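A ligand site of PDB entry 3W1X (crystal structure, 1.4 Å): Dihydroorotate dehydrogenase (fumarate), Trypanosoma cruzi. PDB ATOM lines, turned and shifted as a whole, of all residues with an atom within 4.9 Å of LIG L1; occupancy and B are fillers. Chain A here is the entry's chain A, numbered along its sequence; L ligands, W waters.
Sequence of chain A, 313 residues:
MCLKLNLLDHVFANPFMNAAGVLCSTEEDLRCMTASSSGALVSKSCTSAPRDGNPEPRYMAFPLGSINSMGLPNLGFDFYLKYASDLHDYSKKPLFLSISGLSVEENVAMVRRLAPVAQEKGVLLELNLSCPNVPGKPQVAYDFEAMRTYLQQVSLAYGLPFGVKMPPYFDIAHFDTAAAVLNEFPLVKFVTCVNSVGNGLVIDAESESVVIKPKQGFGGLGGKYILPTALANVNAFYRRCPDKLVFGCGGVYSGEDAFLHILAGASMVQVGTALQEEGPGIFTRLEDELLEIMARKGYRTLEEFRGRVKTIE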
ATOM      1  N   ALA A  19       6.751 -19.629  17.925  1.00  0.00           N
ATOM      2  CA  ALA A  19       6.323 -18.302  17.532  1.00  0.00           C
ATOM      3  C   ALA A  19       5.333 -18.381  16.416  1.00  0.00           C
ATOM      4  O   ALA A  19       5.466 -19.217  15.514  1.00  0.00           O
ATOM      5  CB  ALA A  19       7.535 -17.464  17.124  1.00  0.00           C
ATOM      6  N   ALA A  20       4.333 -17.541  16.383  1.00  0.00           N
ATOM      7  CA  ALA A  20       3.352 -17.595  15.339  1.00  0.00           C
ATOM      8  C   ALA A  20       4.039 -17.451  14.001  1.00  0.00           C
ATOM      9  O   ALA A  20       4.973 -16.678  13.796  1.00  0.00           O
ATOM     10  CB  ALA A  20       2.277 -16.471  15.506  1.00  0.00           C
ATOM     11  N   GLY A  21       3.585 -18.258  13.043  1.00  0.00           N
ATOM     12  CA  GLY A  21       4.101 -18.376  11.725  1.00  0.00           C
ATOM     13  C   GLY A  21       5.049 -19.485  11.481  1.00  0.00           C
ATOM     14  O   GLY A  21       5.257 -19.840  10.330  1.00  0.00           O
ATOM     15  N   VAL A  22       5.691 -19.968  12.528  1.00  0.00           N
ATOM     16  CA  VAL A  22       6.666 -21.091  12.370  1.00  0.00           C
ATOM     17  C   VAL A  22       6.033 -22.401  12.744  1.00  0.00           C
ATOM     18  O   VAL A  22       5.504 -22.539  13.872  1.00  0.00           O
ATOM     19  CB  VAL A  22       7.906 -20.767  13.186  1.00  0.00           C
ATOM     20  CG1 VAL A  22       8.913 -21.939  13.093  1.00  0.00           C
ATOM     21  CG2 VAL A  22       8.515 -19.500  12.640  1.00  0.00           C
ATOM     22  N   LYS A  44      -0.716 -20.241  12.891  1.00  0.00           N
ATOM     23  CA  LYS A  44      -0.319 -19.206  12.008  1.00  0.00           C
ATOM     24  C   LYS A  44      -1.362 -18.071  12.028  1.00  0.00           C
ATOM     25  O   LYS A  44      -2.542 -18.382  11.903  1.00  0.00           O
ATOM     26  CB  LYS A  44      -0.255 -19.794  10.561  1.00  0.00           C
ATOM     27  CG  LYS A  44      -0.053 -18.745   9.483  1.00  0.00           C
ATOM     28  CD  LYS A  44       1.301 -17.925   9.389  1.00  0.00           C
ATOM     29  CE  LYS A  44       1.348 -16.630   8.505  1.00  0.00           C
ATOM     30  NZ  LYS A  44       2.687 -15.729   8.340  1.00  0.00           N
ATOM     31  N   SER A  45      -0.873 -16.846  12.012  1.00  0.00           N
ATOM     32  CA  SER A  45      -1.831 -15.701  11.945  1.00  0.00           C
ATOM     33  C   SER A  45      -2.683 -15.861  10.701  1.00  0.00           C
ATOM     34  O   SER A  45      -2.203 -16.115   9.626  1.00  0.00           O
ATOM     35  CB  SER A  45      -1.112 -14.426  11.794  1.00  0.00           C
ATOM     36  OG  SER A  45      -0.427 -14.095  13.032  1.00  0.00           O
ATOM     37  N   TYR A  59      11.483 -16.245   2.581  1.00  0.00           N
ATOM     38  CA  TYR A  59      12.157 -16.494   3.848  1.00  0.00           C
ATOM     39  C   TYR A  59      13.558 -16.970   3.587  1.00  0.00           C
ATOM     40  O   TYR A  59      13.713 -17.838   2.798  1.00  0.00           O
ATOM     41  CB  TYR A  59      11.414 -17.587   4.688  1.00  0.00           C
ATOM     42  CG  TYR A  59      12.197 -18.067   5.914  1.00  0.00           C
ATOM     43  CD1 TYR A  59      12.108 -17.401   7.113  1.00  0.00           C
ATOM     44  CD2 TYR A  59      13.044 -19.157   5.841  1.00  0.00           C
ATOM     45  CE1 TYR A  59      12.818 -17.816   8.209  1.00  0.00           C
ATOM     46  CE2 TYR A  59      13.753 -19.559   6.944  1.00  0.00           C
ATOM     47  CZ  TYR A  59      13.647 -18.896   8.128  1.00  0.00           C
ATOM     48  OH  TYR A  59      14.323 -19.317   9.236  1.00  0.00           O
ATOM     49  N   SER A  66      17.208 -14.597  10.547  1.00  0.00           N
ATOM     50  CA  SER A  66      16.402 -14.779   9.369  1.00  0.00           C
ATOM     51  C   SER A  66      15.771 -13.455   8.957  1.00  0.00           C
ATOM     52  O   SER A  66      15.731 -12.466   9.677  1.00  0.00           O
ATOM     53  CB  SER A  66      15.278 -15.788   9.629  1.00  0.00           C
ATOM     54  OG  SER A  66      14.333 -15.207  10.571  1.00  0.00           O
ATOM     55  N   ASN A  68      12.223 -12.297   6.528  1.00  0.00           N
ATOM     56  CA  ASN A  68      11.016 -12.792   5.894  1.00  0.00           C
ATOM     57  C   ASN A  68      10.087 -11.675   5.438  1.00  0.00           C
ATOM     58  O   ASN A  68       9.840 -10.706   6.139  1.00  0.00           O
ATOM     59  CB  ASN A  68      10.215 -13.816   6.753  1.00  0.00           C
ATOM     60  CG  ASN A  68       9.238 -13.170   7.673  1.00  0.00           C
ATOM     61  OD1 ASN A  68       8.079 -12.817   7.259  1.00  0.00           O
ATOM     62  ND2 ASN A  68       9.618 -12.981   8.911  1.00  0.00           N
ATOM     63  N   MET A  70       6.736 -12.902   4.210  1.00  0.00           N
ATOM     64  CA  MET A  70       5.834 -13.997   3.836  1.00  0.00           C
ATOM     65  C   MET A  70       4.559 -13.515   3.184  1.00  0.00           C
ATOM     66  O   MET A  70       4.039 -14.122   2.233  1.00  0.00           O
ATOM     67  CB  MET A  70       5.487 -14.835   5.031  1.00  0.00           C
ATOM     68  CG  MET A  70       6.576 -15.451   5.804  1.00  0.00           C
ATOM     69  SD  MET A  70       7.712 -16.489   4.821  1.00  0.00           S
ATOM     70  CE  MET A  70       6.738 -17.886   4.578  1.00  0.00           C
ATOM     71  N   LEU A  72       1.572 -13.088   4.881  1.00  0.00           N
ATOM     72  CA  LEU A  72       0.428 -13.713   5.538  1.00  0.00           C
ATOM     73  C   LEU A  72      -0.131 -14.881   4.743  1.00  0.00           C
ATOM     74  O   LEU A  72      -1.359 -14.989   4.612  1.00  0.00           O
ATOM     75  CB  LEU A  72      -0.691 -12.697   5.841  1.00  0.00           C
ATOM     76  CG  LEU A  72      -0.846 -12.229   7.181  1.00  0.00           C
ATOM     77  CD1 LEU A  72      -1.871 -11.117   7.244  1.00  0.00           C
ATOM     78  CD2 LEU A  72      -1.024 -13.282   8.246  1.00  0.00           C
ATOM     79  N   SER A  98      -3.710 -17.344  16.554  1.00  0.00           N
ATOM     80  CA  SER A  98      -3.312 -15.997  16.195  1.00  0.00           C
ATOM     81  C   SER A  98      -4.181 -15.486  15.043  1.00  0.00           C
ATOM     82  O   SER A  98      -4.407 -16.199  14.058  1.00  0.00           O
ATOM     83  CB  SER A  98      -1.878 -15.974  15.755  1.00  0.00           C
ATOM     84  OG  SER A  98      -1.535 -14.712  15.271  1.00  0.00           O
ATOM     85  N   GLU A 126      -4.379 -14.805  20.416  1.00  0.00           N
ATOM     86  CA  GLU A 126      -3.260 -13.840  20.254  1.00  0.00           C
ATOM     87  C   GLU A 126      -3.617 -12.960  19.083  1.00  0.00           C
ATOM     88  O   GLU A 126      -3.547 -13.406  17.930  1.00  0.00           O
ATOM     89  CB  GLU A 126      -1.904 -14.552  20.091  1.00  0.00           C
ATOM     90  CG  GLU A 126      -0.727 -13.566  20.068  1.00  0.00           C
ATOM     91  CD  GLU A 126       0.635 -14.295  20.033  1.00  0.00           C
ATOM     92  OE1 GLU A 126       1.083 -14.542  18.892  1.00  0.00           O
ATOM     93  OE2 GLU A 126       1.287 -14.574  21.078  1.00  0.00           O
ATOM     94  N   ASN A 128      -2.615 -10.243  16.507  1.00  0.00           N
ATOM     95  CA  ASN A 128      -1.416  -9.673  15.930  1.00  0.00           C
ATOM     96  C   ASN A 128      -1.588  -8.211  15.519  1.00  0.00           C
ATOM     97  O   ASN A 128      -2.240  -7.914  14.623  1.00  0.00           O
ATOM     98  CB  ASN A 128      -1.019 -10.488  14.689  1.00  0.00           C
ATOM     99  CG  ASN A 128       0.337 -10.088  14.097  1.00  0.00           C
ATOM    100  OD1 ASN A 128       1.020  -9.351  14.635  1.00  0.00           O
ATOM    101  ND2 ASN A 128       0.651 -10.657  13.005  1.00  0.00           N
ATOM    102  N   LYS A 165       0.164  -9.540  20.156  1.00  0.00           N
ATOM    103  CA  LYS A 165       1.530  -9.696  19.659  1.00  0.00           C
ATOM    104  C   LYS A 165       1.983  -8.314  19.177  1.00  0.00           C
ATOM    105  O   LYS A 165       1.324  -7.688  18.329  1.00  0.00           O
ATOM    106  CB  LYS A 165       1.544 -10.588  18.451  1.00  0.00           C
ATOM    107  CG  LYS A 165       2.892 -10.908  17.814  1.00  0.00           C
ATOM    108  CD  LYS A 165       3.855 -11.727  18.689  1.00  0.00           C
ATOM    109  CE  LYS A 165       5.069 -12.180  17.886  1.00  0.00           C
ATOM    110  NZ  LYS A 165       4.790 -13.195  16.913  1.00  0.00           N
ATOM    111  N   VAL A 194       8.683 -10.015  21.127  1.00  0.00           N
ATOM    112  CA  VAL A 194       8.310  -9.163  19.996  1.00  0.00           C
ATOM    113  C   VAL A 194       8.145  -9.954  18.688  1.00  0.00           C
ATOM    114  O   VAL A 194       8.572 -11.050  18.519  1.00  0.00           O
ATOM    115  CB  VAL A 194       9.404  -8.072  19.729  1.00  0.00           C
ATOM    116  CG1 VAL A 194       9.490  -7.139  20.916  1.00  0.00           C
ATOM    117  CG2 VAL A 194      10.773  -8.690  19.499  1.00  0.00           C
ATOM    118  N   ASN A 195       7.438  -9.305  17.803  1.00  0.00           N
ATOM    119  CA  ASN A 195       7.411  -9.619  16.370  1.00  0.00           C
ATOM    120  C   ASN A 195       8.792  -9.251  15.744  1.00  0.00           C
ATOM    121  O   ASN A 195       9.630  -8.806  16.411  1.00  0.00           O
ATOM    122  CB  ASN A 195       6.190  -8.933  15.648  1.00  0.00           C
ATOM    123  CG  ASN A 195       5.611  -9.811  14.532  1.00  0.00           C
ATOM    124  OD1 ASN A 195       6.324 -10.277  13.742  1.00  0.00           O
ATOM    125  ND2 ASN A 195       4.320 -10.017  14.544  1.00  0.00           N
ATOM    126  N   SER A 196       8.903  -9.495  14.463  1.00  0.00           N
ATOM    127  CA  SER A 196      10.166  -9.186  13.813  1.00  0.00           C
ATOM    128  C   SER A 196      10.551  -7.726  13.860  1.00  0.00           C
ATOM    129  O   SER A 196       9.760  -6.875  13.903  1.00  0.00           O
ATOM    130  CB  SER A 196      10.239  -9.599  12.342  1.00  0.00           C
ATOM    131  OG  SER A 196       9.094  -9.783  11.726  1.00  0.00           O
ATOM    132  N   GLY A 222      14.515 -11.795  12.326  1.00  0.00           N
ATOM    133  CA  GLY A 222      14.440 -12.590  13.538  1.00  0.00           C
ATOM    134  C   GLY A 222      15.757 -13.224  13.899  1.00  0.00           C
ATOM    135  O   GLY A 222      16.707 -13.099  13.093  1.00  0.00           O
ATOM    136  N   GLY A 223      15.872 -13.881  15.011  1.00  0.00           N
ATOM    137  CA  GLY A 223      17.024 -14.548  15.390  1.00  0.00           C
ATOM    138  C   GLY A 223      18.056 -13.840  16.224  1.00  0.00           C
ATOM    139  O   GLY A 223      17.660 -12.956  17.006  1.00  0.00           O
ATOM    140  N   ILE A 226      18.256 -10.012  17.004  1.00  0.00           N
ATOM    141  CA  ILE A 226      17.176  -9.280  17.679  1.00  0.00           C
ATOM    142  C   ILE A 226      17.070  -9.566  19.162  1.00  0.00           C
ATOM    143  O   ILE A 226      16.205  -9.003  19.810  1.00  0.00           O
ATOM    144  CB  ILE A 226      15.770  -9.454  17.005  1.00  0.00           C
ATOM    145  CG1 ILE A 226      15.068 -10.749  17.305  1.00  0.00           C
ATOM    146  CG2 ILE A 226      15.889  -9.210  15.501  1.00  0.00           C
ATOM    147  CD1 ILE A 226      13.594 -10.670  17.008  1.00  0.00           C
ATOM    148  N   CYS A 249       9.449 -13.315  22.986  1.00  0.00           N
ATOM    149  CA  CYS A 249       9.762 -13.895  21.660  1.00  0.00           C
ATOM    150  C   CYS A 249      10.905 -13.060  21.057  1.00  0.00           C
ATOM    151  O   CYS A 249      10.857 -11.853  21.066  1.00  0.00           O
ATOM    152  CB  CYS A 249       8.519 -13.821  20.752  1.00  0.00           C
ATOM    153  SG  CYS A 249       8.688 -14.673  19.207  1.00  0.00           S
ATOM    154  N   GLY A 250      11.933 -13.712  20.551  1.00  0.00           N
ATOM    155  CA  GLY A 250      12.969 -13.111  19.802  1.00  0.00           C
ATOM    156  C   GLY A 250      14.348 -13.558  20.207  1.00  0.00           C
ATOM    157  O   GLY A 250      14.751 -13.405  21.346  1.00  0.00           O
ATOM    158  N   GLY A 251      15.026 -14.188  19.248  1.00  0.00           N
ATOM    159  CA  GLY A 251      16.395 -14.552  19.512  1.00  0.00           C
ATOM    160  C   GLY A 251      16.658 -15.700  20.417  1.00  0.00           C
ATOM    161  O   GLY A 251      17.789 -15.897  20.883  1.00  0.00           O
ATOM    162  N   VAL A 252      15.639 -16.539  20.637  1.00  0.00           N
ATOM    163  CA  VAL A 252      15.837 -17.750  21.515  1.00  0.00           C
ATOM    164  C   VAL A 252      16.390 -18.914  20.694  1.00  0.00           C
ATOM    165  O   VAL A 252      15.724 -19.450  19.843  1.00  0.00           O
ATOM    166  CB  VAL A 252      14.541 -18.185  22.266  1.00  0.00           C
ATOM    167  CG1 VAL A 252      14.799 -19.452  23.076  1.00  0.00           C
ATOM    168  CG2 VAL A 252      14.055 -17.036  23.162  1.00  0.00           C
ATOM    169  N   GLN A 270       8.580 -17.930  23.354  1.00  0.00           N
ATOM    170  CA  GLN A 270       8.266 -18.408  21.965  1.00  0.00           C
ATOM    171  C   GLN A 270       9.590 -18.506  21.162  1.00  0.00           C
ATOM    172  O   GLN A 270      10.488 -17.670  21.381  1.00  0.00           O
ATOM    173  CB  GLN A 270       7.299 -17.419  21.306  1.00  0.00           C
ATOM    174  CG  GLN A 270       6.077 -17.083  22.148  1.00  0.00           C
ATOM    175  CD  GLN A 270       5.030 -16.356  21.344  1.00  0.00           C
ATOM    176  OE1 GLN A 270       5.341 -15.714  20.377  1.00  0.00           O
ATOM    177  NE2 GLN A 270       3.752 -16.437  21.764  1.00  0.00           N
ATOM    178  N   VAL A 271       9.592 -19.428  20.221  1.00  0.00           N
ATOM    179  CA  VAL A 271      10.763 -19.715  19.419  1.00  0.00           C
ATOM    180  C   VAL A 271      10.381 -19.732  17.980  1.00  0.00           C
ATOM    181  O   VAL A 271       9.516 -20.544  17.536  1.00  0.00           O
ATOM    182  CB  VAL A 271      11.312 -21.118  19.854  1.00  0.00           C
ATOM    183  CG1 VAL A 271      12.649 -21.310  19.156  1.00  0.00           C
ATOM    184  CG2 VAL A 271      11.476 -21.211  21.406  1.00  0.00           C
ATOM    185  N   GLY A 272      10.959 -18.810  17.204  1.00  0.00           N
ATOM    186  CA  GLY A 272      10.695 -18.644  15.761  1.00  0.00           C
ATOM    187  C   GLY A 272      11.809 -19.224  14.914  1.00  0.00           C
ATOM    188  O   GLY A 272      11.822 -20.392  14.607  1.00  0.00           O
ATOM    189  N   THR A 273      12.700 -18.320  14.518  1.00  0.00           N
ATOM    190  CA  THR A 273      13.849 -18.672  13.664  1.00  0.00           C
ATOM    191  C   THR A 273      14.510 -19.966  14.079  1.00  0.00           C
ATOM    192  O   THR A 273      14.743 -20.787  13.225  1.00  0.00           O
ATOM    193  CB  THR A 273      14.842 -17.504  13.612  1.00  0.00           C
ATOM    194  OG1 THR A 273      14.193 -16.326  13.089  1.00  0.00           O
ATOM    195  CG2 THR A 273      16.005 -17.815  12.710  1.00  0.00           C
ATOM    196  N   ALA A 274      14.877 -20.081  15.345  1.00  0.00           N
ATOM    197  CA  ALA A 274      15.671 -21.263  15.699  1.00  0.00           C
ATOM    198  C   ALA A 274      14.879 -22.550  15.554  1.00  0.00           C
ATOM    199  O   ALA A 274      15.421 -23.611  15.223  1.00  0.00           O
ATOM    200  CB  ALA A 274      16.126 -21.161  17.173  1.00  0.00           C
HETATM  201  N1  LIG L   1       4.486 -13.378  13.760  1.00  0.00           N
HETATM  202  C1  LIG L   1       3.117 -13.336  13.836  1.00  0.00           C
HETATM  203  O1  LIG L   1       2.647 -12.836  14.882  1.00  0.00           O
HETATM  204  N2  LIG L   1       2.318 -13.892  12.921  1.00  0.00           N
HETATM  205  C2  LIG L   1       2.805 -14.543  11.880  1.00  0.00           C
HETATM  206  O2  LIG L   1       2.022 -15.093  11.057  1.00  0.00           O
HETATM  207  C3  LIG L   1       4.224 -14.584  11.664  1.00  0.00           C
HETATM  208  N3  LIG L   1       4.766 -15.209  10.627  1.00  0.00           N
HETATM  209  C4  LIG L   1       6.128 -15.492  10.602  1.00  0.00           C
HETATM  210  C5  LIG L   1       6.667 -16.260   9.589  1.00  0.00           C
HETATM  211  C6  LIG L   1       8.002 -16.542   9.541  1.00  0.00           C
HETATM  212  C7  LIG L   1       8.640 -17.397   8.469  1.00  0.00           C
HETATM  213  C8  LIG L   1       8.878 -15.992  10.561  1.00  0.00           C
HETATM  214  C9  LIG L   1      10.373 -16.243  10.579  1.00  0.00           C
HETATM  215  C10 LIG L   1       8.322 -15.186  11.558  1.00  0.00           C
HETATM  216  C11 LIG L   1       6.950 -14.926  11.604  1.00  0.00           C
HETATM  217  N4  LIG L   1       6.376 -14.082  12.616  1.00  0.00           N
HETATM  218  C12 LIG L   1       5.014 -14.018  12.700  1.00  0.00           C
HETATM  219  C13 LIG L   1       7.236 -13.531  13.698  1.00  0.00           C
HETATM  220  C14 LIG L   1       7.659 -14.547  14.714  1.00  0.00           C
HETATM  221  O3  LIG L   1       6.450 -14.955  15.407  1.00  0.00           O
HETATM  222  C15 LIG L   1       8.554 -13.924  15.715  1.00  0.00           C
HETATM  223  O4  LIG L   1       7.892 -12.828  16.366  1.00  0.00           O
HETATM  224  C16 LIG L   1       9.871 -13.381  15.109  1.00  0.00           C
HETATM  225  O5  LIG L   1      10.353 -14.326  14.126  1.00  0.00           O
HETATM  226  C17 LIG L   1      10.974 -13.209  16.148  1.00  0.00           C
HETATM  227  O6  LIG L   1      11.282 -14.388  16.871  1.00  0.00           O
HETATM  228  P1  LIG L   1      12.624 -15.232  16.506  1.00  0.00           P
HETATM  229  O7  LIG L   1      12.553 -16.453  17.411  1.00  0.00           O
HETATM  230  O8  LIG L   1      13.797 -14.337  16.771  1.00  0.00           O
HETATM  231  O9  LIG L   1      12.507 -15.567  14.983  1.00  0.00           O
HETATM  232  O1  LG2 L   2       4.992 -11.657   6.472  1.00  0.00           O
HETATM  233  C1  LG2 L   2       4.281 -12.232   7.297  1.00  0.00           C
HETATM  234  O2  LG2 L   2       3.332 -13.047   7.082  1.00  0.00           O
HETATM  235  C2  LG2 L   2       4.558 -11.897   8.787  1.00  0.00           C
HETATM  236  N1  LG2 L   2       5.920 -12.044   9.090  1.00  0.00           N
HETATM  237  C3  LG2 L   2       6.421 -11.670  10.282  1.00  0.00           C
HETATM  238  O3  LG2 L   2       7.608 -11.777  10.562  1.00  0.00           O
HETATM  239  N2  LG2 L   2       5.477 -11.283  11.227  1.00  0.00           N
HETATM  240  C4  LG2 L   2       4.074 -11.173  11.013  1.00  0.00           C
HETATM  241  O4  LG2 L   2       3.338 -10.808  11.962  1.00  0.00           O
HETATM  242  C5  LG2 L   2       3.612 -11.569   9.730  1.00  0.00           C
HETATM  243  C6  LG2 L   2       2.209 -11.392   9.446  1.00  0.00           C
HETATM  244  C7  LG2 L   2       1.764  -9.890   9.353  1.00  0.00           C
HETATM  245  C8  LG2 L   2       2.387  -9.242   8.256  1.00  0.00           C
HETATM  246  C9  LG2 L   2       1.837  -9.221   6.977  1.00  0.00           C
HETATM  247  C10 LG2 L   2       2.598  -8.634   5.872  1.00  0.00           C
HETATM  248  C11 LG2 L   2       3.809  -8.055   6.047  1.00  0.00           C
HETATM  249  C12 LG2 L   2       4.621  -7.419   4.947  1.00  0.00           C
HETATM  250  C13 LG2 L   2       5.188  -8.597   4.126  1.00  0.00           C
HETATM  251  N3  LG2 L   2       5.617  -9.483   3.579  1.00  0.00           N
HETATM  252  C14 LG2 L   2       4.318  -7.975   7.354  1.00  0.00           C
HETATM  253  C15 LG2 L   2       3.600  -8.563   8.419  1.00  0.00           C
HETATM  254  O   HOH W   1      12.644 -16.450  20.088  1.00  0.00           O
HETATM  255  O   HOH W   2       0.355 -13.379  16.579  1.00  0.00           O
HETATM  256  O   HOH W   3      14.705 -18.129  17.395  1.00  0.00           O
HETATM  257  O   HOH W   4      10.906 -12.541  12.064  1.00  0.00           O
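The side-chain amino group of Lys 44 is in salt-bridge range of an oxygen (O2) of LG2 L2.
An oxygen (O9) of LIG L1 lies within hydrogen-bond range of the side-chain hydroxyl (OG1) of Thr 273 (2.6 Å).
N of Gly 223 sits at hydrogen-bond distance from O8 of LIG L1 (2.8 Å).
An oxygen (O7) of LIG L1 lies within hydrogen-bond range of the backbone NH (N) of Gly 272 (2.9 Å).
O9 of LIG L1 is in hydrogen-bond range of N of Thr 273, 2.8 Å away.
ND2 of Asn 195 lies within hydrogen-bond range of O1 of LIG L1.
NZ of Lys 165 sits at hydrogen-bond distance from O3 of LIG L1.
N of Met 70 sits at hydrogen-bond distance from O1 of LG2 L2.
OD1 of Asn 195 lies within hydrogen-bond range of N2 of LG2 L2 (2.8 Å).
The side-chain hydroxyl (OG) of Ser 196 sits at hydrogen-bond distance from an oxygen (O3) of LG2 L2 (2.7 Å).
The side-chain amino group (NZ) of Lys 44 is in hydrogen-bond range of an oxygen (O2) of LIG L1, 2.9 Å away.
The backbone NH (N) of Ala 20 is in hydrogen-bond range of an oxygen (O3) of LIG L1 (3.5 Å).
The side-chain sulfur (SG) of Cys 249 is in hydrogen-bond range of an oxygen (O4) of LIG L1, 3.5 Å away.
The side-chain amide nitrogen (ND2) of Asn 68 lies within hydrogen-bond range of an oxygen (O3) of LG2 L2 (2.9 Å).
A nitrogen (N2) of LIG L1 lies within hydrogen-bond range of the side-chain hydroxyl (OG) of Ser 45, 2.8 Å away.
An oxygen (O4) of LIG L1 lies within hydrogen-bond range of the backbone carbonyl oxygen (O) of Val 194 (2.9 Å).
An oxygen (O3) of LIG L1 sits at hydrogen-bond distance from the backbone carbonyl oxygen (O) of Ala 20, at 2.8 Å.
An oxygen (O4) of LG2 L2 sits at hydrogen-bond distance from the side-chain amide nitrogen of Asn 128.
The backbone NH (N) of Leu 72 lies within hydrogen-bond range of an oxygen (O2) of LG2 L2 (2.8 Å).
N of Gly 251 lies within hydrogen-bond range of O8 of LIG L1, at 2.8 Å.
Residues that only touch LIG L1: Ala 19 (3.2 Å), Gly 250 (3.4 Å), Gly 21 (3.4 Å), Asn 128 (3.5 Å), Asn 68 (3.5 Å), Gly 222 (3.7 Å), Ile 226 (3.7 Å), Tyr 59 (3.7 Å), Met 70 (3.9 Å), Ser 196 (3.97 Å) and Val 271 (3.97 Å).
Hydrophobic or aromatic side chains that line LIG L1: Ala 19, Ala 20, Tyr 59, Met 70 and Ile 226.
An oxygen (O4) of LG2 L2 lies close to a nitrogen (N2) of LIG L1 (3.4 Å).
Water W3 lies within hydrogen-bond range of an oxygen (O7) of LIG L1 (2.7 Å), the backbone NH of Ala 274 (2.8 Å) and the backbone carbonyl oxygen of Val 252 (3.0 Å).
Water W4 lies within hydrogen-bond range of O5 of LIG L1 (2.8 Å), OG of Ser 196 (3.3 Å) and ND2 of Asn 68 (3.4 Å).
Water W2 lies within hydrogen-bond range of the side-chain hydroxyl (OG) of Ser 98 (2.7 Å), the side-chain carboxylate (OE1) of Glu 126 (2.7 Å) and an oxygen (O1) of LIG L1 (2.9 Å).
The side-chain hydroxyl of Thr 273 sits at hydrogen-bond distance from the side-chain hydroxyl of Ser 66 (2.8 Å).
The backbone NH of Gly 222 lies within hydrogen-bond range of the backbone carbonyl oxygen of Ser 66, at 3.0 Å.
The side-chain sulfur (SG) of Cys 249 sits at hydrogen-bond distance from the side-chain amide oxygen (OE1) of Gln 270 (3.7 Å).
OG of Ser 196 lies within hydrogen-bond range of OD1 of Asn 195 (3.5 Å).
OD1 of Asn 68 lies within hydrogen-bond range of N of Met 70.
The backbone carbonyl oxygen of Cys 249 sits at hydrogen-bond distance from the backbone NH of Val 194.
The side-chain hydroxyl of Ser 45 is in hydrogen-bond range of the side-chain hydroxyl of Ser 98 (2.6 Å).
The side-chain amide nitrogen (ND2) of Asn 195 is in hydrogen-bond range of the side-chain amide oxygen (OD1) of Asn 128, 3.4 Å away.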
